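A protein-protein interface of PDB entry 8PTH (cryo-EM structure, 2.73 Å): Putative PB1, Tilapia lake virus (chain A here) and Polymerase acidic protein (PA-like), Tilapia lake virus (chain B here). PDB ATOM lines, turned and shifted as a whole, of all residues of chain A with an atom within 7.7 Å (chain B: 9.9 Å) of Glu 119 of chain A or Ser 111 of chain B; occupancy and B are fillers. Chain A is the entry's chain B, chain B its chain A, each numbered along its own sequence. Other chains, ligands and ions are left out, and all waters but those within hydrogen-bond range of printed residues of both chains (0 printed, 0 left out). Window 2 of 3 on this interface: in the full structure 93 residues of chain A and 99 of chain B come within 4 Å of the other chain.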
ATOM      1  N   LYS A 114     -10.140  13.710  18.738  1.00  0.00           N
ATOM      2  CA  LYS A 114     -10.659  13.901  20.087  1.00  0.00           C
ATOM      3  C   LYS A 114     -11.645  12.803  20.459  1.00  0.00           C
ATOM      4  O   LYS A 114     -11.600  12.269  21.572  1.00  0.00           O
ATOM      5  CB  LYS A 114     -11.316  15.276  20.204  1.00  0.00           C
ATOM      6  CG  LYS A 114     -10.416  16.335  20.820  1.00  0.00           C
ATOM      7  CD  LYS A 114     -10.753  17.733  20.322  1.00  0.00           C
ATOM      8  CE  LYS A 114     -11.113  18.658  21.472  1.00  0.00           C
ATOM      9  NZ  LYS A 114     -11.303  20.064  21.018  1.00  0.00           N
ATOM     10  N   VAL A 115     -12.540  12.445  19.535  1.00  0.00           N
ATOM     11  CA  VAL A 115     -13.523  11.403  19.818  1.00  0.00           C
ATOM     12  C   VAL A 115     -12.824  10.083  20.104  1.00  0.00           C
ATOM     13  O   VAL A 115     -13.201   9.351  21.028  1.00  0.00           O
ATOM     14  CB  VAL A 115     -14.517  11.278  18.649  1.00  0.00           C
ATOM     15  CG1 VAL A 115     -15.243   9.944  18.701  1.00  0.00           C
ATOM     16  CG2 VAL A 115     -15.508  12.428  18.673  1.00  0.00           C
ATOM     17  N   LEU A 116     -11.801   9.752  19.320  1.00  0.00           N
ATOM     18  CA  LEU A 116     -11.074   8.507  19.520  1.00  0.00           C
ATOM     19  C   LEU A 116     -10.136   8.550  20.719  1.00  0.00           C
ATOM     20  O   LEU A 116      -9.680   7.490  21.161  1.00  0.00           O
ATOM     21  CB  LEU A 116     -10.272   8.159  18.265  1.00  0.00           C
ATOM     22  CG  LEU A 116     -11.079   7.661  17.066  1.00  0.00           C
ATOM     23  CD1 LEU A 116     -10.191   7.556  15.839  1.00  0.00           C
ATOM     24  CD2 LEU A 116     -11.733   6.324  17.370  1.00  0.00           C
ATOM     25  N   THR A 117      -9.837   9.734  21.254  1.00  0.00           N
ATOM     26  CA  THR A 117      -8.850   9.869  22.317  1.00  0.00           C
ATOM     27  C   THR A 117      -9.460   9.977  23.711  1.00  0.00           C
ATOM     28  O   THR A 117      -8.768   9.677  24.691  1.00  0.00           O
ATOM     29  CB  THR A 117      -7.969  11.099  22.050  1.00  0.00           C
ATOM     30  OG1 THR A 117      -7.019  10.788  21.022  1.00  0.00           O
ATOM     31  CG2 THR A 117      -7.216  11.530  23.303  1.00  0.00           C
ATOM     32  N   VAL A 118     -10.727  10.379  23.832  1.00  0.00           N
ATOM     33  CA  VAL A 118     -11.315  10.553  25.155  1.00  0.00           C
ATOM     34  C   VAL A 118     -11.248   9.240  25.928  1.00  0.00           C
ATOM     35  O   VAL A 118     -11.197   8.148  25.349  1.00  0.00           O
ATOM     36  CB  VAL A 118     -12.766  11.055  25.065  1.00  0.00           C
ATOM     37  CG1 VAL A 118     -12.817  12.432  24.428  1.00  0.00           C
ATOM     38  CG2 VAL A 118     -13.630  10.069  24.296  1.00  0.00           C
ATOM     39  N   GLU A 119     -11.248   9.351  27.255  1.00  0.00           N
ATOM     40  CA  GLU A 119     -11.142   8.200  28.140  1.00  0.00           C
ATOM     41  C   GLU A 119     -12.487   7.728  28.673  1.00  0.00           C
ATOM     42  O   GLU A 119     -12.528   6.761  29.439  1.00  0.00           O
ATOM     43  CB  GLU A 119     -10.215   8.528  29.313  1.00  0.00           C
ATOM     44  CG  GLU A 119     -10.810   9.514  30.307  1.00  0.00           C
ATOM     45  CD  GLU A 119      -9.810  10.549  30.784  1.00  0.00           C
ATOM     46  OE1 GLU A 119      -8.591  10.287  30.705  1.00  0.00           O
ATOM     47  OE2 GLU A 119     -10.245  11.629  31.238  1.00  0.00           O
ATOM     48  N   SER A 120     -13.584   8.381  28.298  1.00  0.00           N
ATOM     49  CA  SER A 120     -14.902   7.977  28.765  1.00  0.00           C
ATOM     50  C   SER A 120     -15.948   8.498  27.793  1.00  0.00           C
ATOM     51  O   SER A 120     -15.705   9.443  27.038  1.00  0.00           O
ATOM     52  CB  SER A 120     -15.176   8.494  30.181  1.00  0.00           C
ATOM     53  OG  SER A 120     -16.401   7.988  30.681  1.00  0.00           O
ATOM     54  N   LEU A 121     -17.120   7.863  27.821  1.00  0.00           N
ATOM     55  CA  LEU A 121     -18.221   8.282  26.964  1.00  0.00           C
ATOM     56  C   LEU A 121     -18.896   9.553  27.456  1.00  0.00           C
ATOM     57  O   LEU A 121     -19.547  10.239  26.662  1.00  0.00           O
ATOM     58  CB  LEU A 121     -19.258   7.162  26.857  1.00  0.00           C
ATOM     59  CG  LEU A 121     -18.858   5.956  26.007  1.00  0.00           C
ATOM     60  CD1 LEU A 121     -19.866   4.833  26.174  1.00  0.00           C
ATOM     61  CD2 LEU A 121     -18.728   6.340  24.542  1.00  0.00           C
ATOM     62  N   SER A 122     -18.762   9.880  28.739  1.00  0.00           N
ATOM     63  CA  SER A 122     -19.338  11.094  29.301  1.00  0.00           C
ATOM     64  C   SER A 122     -18.358  12.260  29.328  1.00  0.00           C
ATOM     65  O   SER A 122     -18.747  13.368  29.710  1.00  0.00           O
ATOM     66  CB  SER A 122     -19.849  10.825  30.719  1.00  0.00           C
ATOM     67  OG  SER A 122     -18.975   9.959  31.420  1.00  0.00           O
ATOM     68  N   GLU A 123     -17.103  12.042  28.938  1.00  0.00           N
ATOM     69  CA  GLU A 123     -16.132  13.126  28.926  1.00  0.00           C
ATOM     70  C   GLU A 123     -16.548  14.199  27.928  1.00  0.00           C
ATOM     71  O   GLU A 123     -17.059  13.900  26.846  1.00  0.00           O
ATOM     72  CB  GLU A 123     -14.744  12.588  28.577  1.00  0.00           C
ATOM     73  CG  GLU A 123     -13.725  13.671  28.263  1.00  0.00           C
ATOM     74  CD  GLU A 123     -12.294  13.188  28.403  1.00  0.00           C
ATOM     75  OE1 GLU A 123     -12.050  12.269  29.211  1.00  0.00           O
ATOM     76  OE2 GLU A 123     -11.412  13.729  27.703  1.00  0.00           O
ATOM     77  N   VAL A 130     -19.078  11.977  23.670  1.00  0.00           N
ATOM     78  CA  VAL A 130     -19.202  10.853  22.744  1.00  0.00           C
ATOM     79  C   VAL A 130     -20.550  10.171  22.920  1.00  0.00           C
ATOM     80  O   VAL A 130     -21.166   9.720  21.947  1.00  0.00           O
ATOM     81  CB  VAL A 130     -18.038   9.866  22.936  1.00  0.00           C
ATOM     82  CG1 VAL A 130     -18.221   8.648  22.042  1.00  0.00           C
ATOM     83  CG2 VAL A 130     -16.718  10.546  22.642  1.00  0.00           C
ATOM     84  N   SER A 237     -12.340   1.324  16.583  1.00  0.00           N
ATOM     85  CA  SER A 237     -13.508   1.825  17.299  1.00  0.00           C
ATOM     86  C   SER A 237     -14.464   2.597  16.399  1.00  0.00           C
ATOM     87  O   SER A 237     -15.644   2.724  16.739  1.00  0.00           O
ATOM     88  CB  SER A 237     -13.064   2.715  18.459  1.00  0.00           C
ATOM     89  OG  SER A 237     -12.552   1.937  19.525  1.00  0.00           O
ATOM     90  N   HIS B 108      -7.328   2.361  15.304  1.00  0.00           N
ATOM     91  CA  HIS B 108      -7.239   2.824  16.681  1.00  0.00           C
ATOM     92  C   HIS B 108      -8.399   2.287  17.507  1.00  0.00           C
ATOM     93  O   HIS B 108      -9.551   2.282  17.064  1.00  0.00           O
ATOM     94  CB  HIS B 108      -7.231   4.352  16.719  1.00  0.00           C
ATOM     95  CG  HIS B 108      -7.083   4.924  18.094  1.00  0.00           C
ATOM     96  ND1 HIS B 108      -5.875   5.349  18.599  1.00  0.00           N
ATOM     97  CD2 HIS B 108      -7.996   5.142  19.071  1.00  0.00           C
ATOM     98  CE1 HIS B 108      -6.047   5.804  19.827  1.00  0.00           C
ATOM     99  NE2 HIS B 108      -7.325   5.689  20.137  1.00  0.00           N
ATOM    100  N   LYS B 109      -8.089   1.835  18.719  1.00  0.00           N
ATOM    101  CA  LYS B 109      -9.078   1.303  19.647  1.00  0.00           C
ATOM    102  C   LYS B 109      -9.257   2.292  20.790  1.00  0.00           C
ATOM    103  O   LYS B 109      -8.294   2.611  21.495  1.00  0.00           O
ATOM    104  CB  LYS B 109      -8.647  -0.064  20.180  1.00  0.00           C
ATOM    105  CG  LYS B 109      -9.647  -0.706  21.125  1.00  0.00           C
ATOM    106  CD  LYS B 109      -9.119  -2.014  21.687  1.00  0.00           C
ATOM    107  CE  LYS B 109     -10.017  -2.543  22.793  1.00  0.00           C
ATOM    108  NZ  LYS B 109      -9.466  -3.772  23.425  1.00  0.00           N
ATOM    109  N   ALA B 110     -10.484   2.771  20.971  1.00  0.00           N
ATOM    110  CA  ALA B 110     -10.778   3.712  22.037  1.00  0.00           C
ATOM    111  C   ALA B 110     -10.977   2.979  23.360  1.00  0.00           C
ATOM    112  O   ALA B 110     -11.190   1.765  23.407  1.00  0.00           O
ATOM    113  CB  ALA B 110     -12.023   4.532  21.701  1.00  0.00           C
ATOM    114  N   SER B 111     -10.905   3.743  24.452  1.00  0.00           N
ATOM    115  CA  SER B 111     -11.081   3.168  25.780  1.00  0.00           C
ATOM    116  C   SER B 111     -12.492   2.636  25.999  1.00  0.00           C
ATOM    117  O   SER B 111     -12.697   1.822  26.905  1.00  0.00           O
ATOM    118  CB  SER B 111     -10.749   4.211  26.848  1.00  0.00           C
ATOM    119  OG  SER B 111     -11.775   5.184  26.947  1.00  0.00           O
ATOM    120  N   TYR B 112     -13.460   3.072  25.198  1.00  0.00           N
ATOM    121  CA  TYR B 112     -14.846   2.643  25.329  1.00  0.00           C
ATOM    122  C   TYR B 112     -15.229   1.582  24.305  1.00  0.00           C
ATOM    123  O   TYR B 112     -16.419   1.292  24.144  1.00  0.00           O
ATOM    124  CB  TYR B 112     -15.786   3.846  25.206  1.00  0.00           C
ATOM    125  CG  TYR B 112     -15.482   4.744  24.030  1.00  0.00           C
ATOM    126  CD1 TYR B 112     -15.957   4.444  22.761  1.00  0.00           C
ATOM    127  CD2 TYR B 112     -14.713   5.889  24.187  1.00  0.00           C
ATOM    128  CE1 TYR B 112     -15.679   5.260  21.685  1.00  0.00           C
ATOM    129  CE2 TYR B 112     -14.430   6.711  23.116  1.00  0.00           C
ATOM    130  CZ  TYR B 112     -14.915   6.392  21.867  1.00  0.00           C
ATOM    131  OH  TYR B 112     -14.635   7.208  20.797  1.00  0.00           O
ATOM    132  N   ASP B 113     -14.251   0.997  23.610  1.00  0.00           N
ATOM    133  CA  ASP B 113     -14.565  -0.008  22.600  1.00  0.00           C
ATOM    134  C   ASP B 113     -15.274  -1.207  23.216  1.00  0.00           C
ATOM    135  O   ASP B 113     -16.264  -1.703  22.665  1.00  0.00           O
ATOM    136  CB  ASP B 113     -13.281  -0.449  21.893  1.00  0.00           C
ATOM    137  CG  ASP B 113     -13.552  -1.264  20.645  1.00  0.00           C
ATOM    138  OD1 ASP B 113     -14.252  -2.293  20.743  1.00  0.00           O
ATOM    139  OD2 ASP B 113     -13.062  -0.877  19.565  1.00  0.00           O
ATOM    140  N   ALA B 114     -14.784  -1.684  24.362  1.00  0.00           N
ATOM    141  CA  ALA B 114     -15.399  -2.842  25.001  1.00  0.00           C
ATOM    142  C   ALA B 114     -16.825  -2.539  25.442  1.00  0.00           C
ATOM    143  O   ALA B 114     -17.718  -3.379  25.294  1.00  0.00           O
ATOM    144  CB  ALA B 114     -14.554  -3.290  26.194  1.00  0.00           C
ATOM    145  N   GLU B 115     -17.058  -1.346  25.993  1.00  0.00           N
ATOM    146  CA  GLU B 115     -18.401  -0.993  26.441  1.00  0.00           C
ATOM    147  C   GLU B 115     -19.378  -0.942  25.272  1.00  0.00           C
ATOM    148  O   GLU B 115     -20.498  -1.461  25.363  1.00  0.00           O
ATOM    149  CB  GLU B 115     -18.368   0.348  27.173  1.00  0.00           C
ATOM    150  CG  GLU B 115     -19.718   1.030  27.288  1.00  0.00           C
ATOM    151  CD  GLU B 115     -19.746   2.079  28.381  1.00  0.00           C
ATOM    152  OE1 GLU B 115     -18.660   2.522  28.807  1.00  0.00           O
ATOM    153  OE2 GLU B 115     -20.854   2.462  28.810  1.00  0.00           O
ATOM    154  N   LEU B 116     -18.973  -0.321  24.163  1.00  0.00           N
ATOM    155  CA  LEU B 116     -19.848  -0.257  22.997  1.00  0.00           C
ATOM    156  C   LEU B 116     -20.089  -1.643  22.416  1.00  0.00           C
ATOM    157  O   LEU B 116     -21.200  -1.952  21.972  1.00  0.00           O
ATOM    158  CB  LEU B 116     -19.251   0.672  21.941  1.00  0.00           C
ATOM    159  CG  LEU B 116     -19.271   2.169  22.258  1.00  0.00           C
ATOM    160  CD1 LEU B 116     -18.695   2.958  21.096  1.00  0.00           C
ATOM    161  CD2 LEU B 116     -20.675   2.651  22.585  1.00  0.00           C
ATOM    162  N   ARG B 117     -19.059  -2.493  22.399  1.00  0.00           N
ATOM    163  CA  ARG B 117     -19.246  -3.856  21.912  1.00  0.00           C
ATOM    164  C   ARG B 117     -20.222  -4.624  22.794  1.00  0.00           C
ATOM    165  O   ARG B 117     -21.058  -5.385  22.292  1.00  0.00           O
ATOM    166  CB  ARG B 117     -17.901  -4.575  21.838  1.00  0.00           C
ATOM    167  CG  ARG B 117     -17.334  -4.660  20.431  1.00  0.00           C
ATOM    168  CD  ARG B 117     -15.961  -5.306  20.419  1.00  0.00           C
ATOM    169  NE  ARG B 117     -15.020  -4.583  19.572  1.00  0.00           N
ATOM    170  CZ  ARG B 117     -14.979  -4.671  18.249  1.00  0.00           C
ATOM    171  NH1 ARG B 117     -15.826  -5.435  17.581  1.00  0.00           N
ATOM    172  NH2 ARG B 117     -14.063  -3.976  17.581  1.00  0.00           N
ATOM    173  N   GLU B 118     -20.130  -4.445  24.113  1.00  0.00           N
ATOM    174  CA  GLU B 118     -21.082  -5.086  25.014  1.00  0.00           C
ATOM    175  C   GLU B 118     -22.497  -4.587  24.757  1.00  0.00           C
ATOM    176  O   GLU B 118     -23.451  -5.376  24.736  1.00  0.00           O
ATOM    177  CB  GLU B 118     -20.684  -4.829  26.466  1.00  0.00           C
ATOM    178  CG  GLU B 118     -19.644  -5.791  27.005  1.00  0.00           C
ATOM    179  CD  GLU B 118     -19.062  -5.335  28.329  1.00  0.00           C
ATOM    180  OE1 GLU B 118     -19.833  -5.191  29.301  1.00  0.00           O
ATOM    181  OE2 GLU B 118     -17.834  -5.120  28.399  1.00  0.00           O
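O of Leu 121 of chain A lies within hydrogen-bond range of N of Val 130 of chain A, 3.5 Å away. The guanidinium group of Arg 117 of chain B is in salt-bridge range of the side-chain carboxylate of Asp 113 of chain B, 2.7 Å away. OG of Ser 120 of chain A is in hydrogen-bond range of OG of Ser 122 of chain A.
NE2 of His 108 of chain B is in hydrogen-bond range of O of Leu 116 of chain A (3.1 Å). O of Glu 119 of chain A is in hydrogen-bond range of OG of Ser 111 of chain B, 3.0 Å away. The side-chain hydroxyl of Ser 237 of chain A is in hydrogen-bond range of the backbone NH of Ala 110 of chain B, 2.7 Å away. The side-chain hydroxyl (OG) of Ser 237 of chain A is in hydrogen-bond range of the side-chain carboxylate (OD2) of Asp 113 of chain B. The backbone carbonyl oxygen (O) of Val 115 of chain A is in hydrogen-bond range of the side-chain hydroxyl (OH) of Tyr 112 of chain B (2.6 Å). O of His 108 of chain B lies within hydrogen-bond range of N of Ser 237 of chain A (3.0 Å). The side-chain hydroxyl (OG) of Ser 111 of chain B sits at hydrogen-bond distance from the backbone carbonyl oxygen (O) of Val 118 of chain A (3.4 Å).
Of the 11 printed residues of chain B, 7 touch a printed residue of chain A. Hydrophobic or aromatic side chains of chain B that line the printed part of chain A: His 108, Ala 110 and Tyr 112. Among the printed residues, no Asp or Glu carboxylate lies within 4 Å of a Lys or Arg side-chain nitrogen of the other chain.
Among the printed residues, pairs that only touch across the chains: Leu 116 of chain A with Ala 110 of chain B (3.8 Å), Leu 116 of chain A with Tyr 112 of chain B (3.9999 Å), Val 118 of chain A with Tyr 112 of chain B (3.6 Å), Ser 120 of chain A with Ser 111 of chain B (3.9 Å), Leu 121 of chain A with Tyr 112 of chain B (3.7 Å), Leu 121 of chain A with Glu 115 of chain B (3.5 Å) and Ser 237 of chain A with Lys 109 of chain B (3.5 Å).
Lys 114 of chain A touches none of the printed residues of chain B. Printed residues of chain B within 4 Å of Val 115 of chain A: Tyr 112 (2.6 Å). Printed residues of chain B within 4 Å of Leu 116 of chain A: His 108, Ala 110 and Tyr 112. Printed residues of chain B within 4 Å of Glu 119 of chain A: Ser 111 (3.0 Å). Printed residues of chain B within 4 Å of Leu 121 of chain A: Tyr 112 and Glu 115. Printed residues of chain A within 4 Å of Ser 111 of chain B: Val 118 (3.4 Å), Glu 119 (3.0 Å) and Ser 120 (3.9 Å). Arg 117 of chain B touches none of the printed residues of chain A. The nearest residue of chain A that does not touch Ser 111 of chain B is Leu 116 of chain A (5.1 Å). The nearest printed residue of chain B that does not touch Val 115 of chain A is Ala 110 of chain B (5.0 Å).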
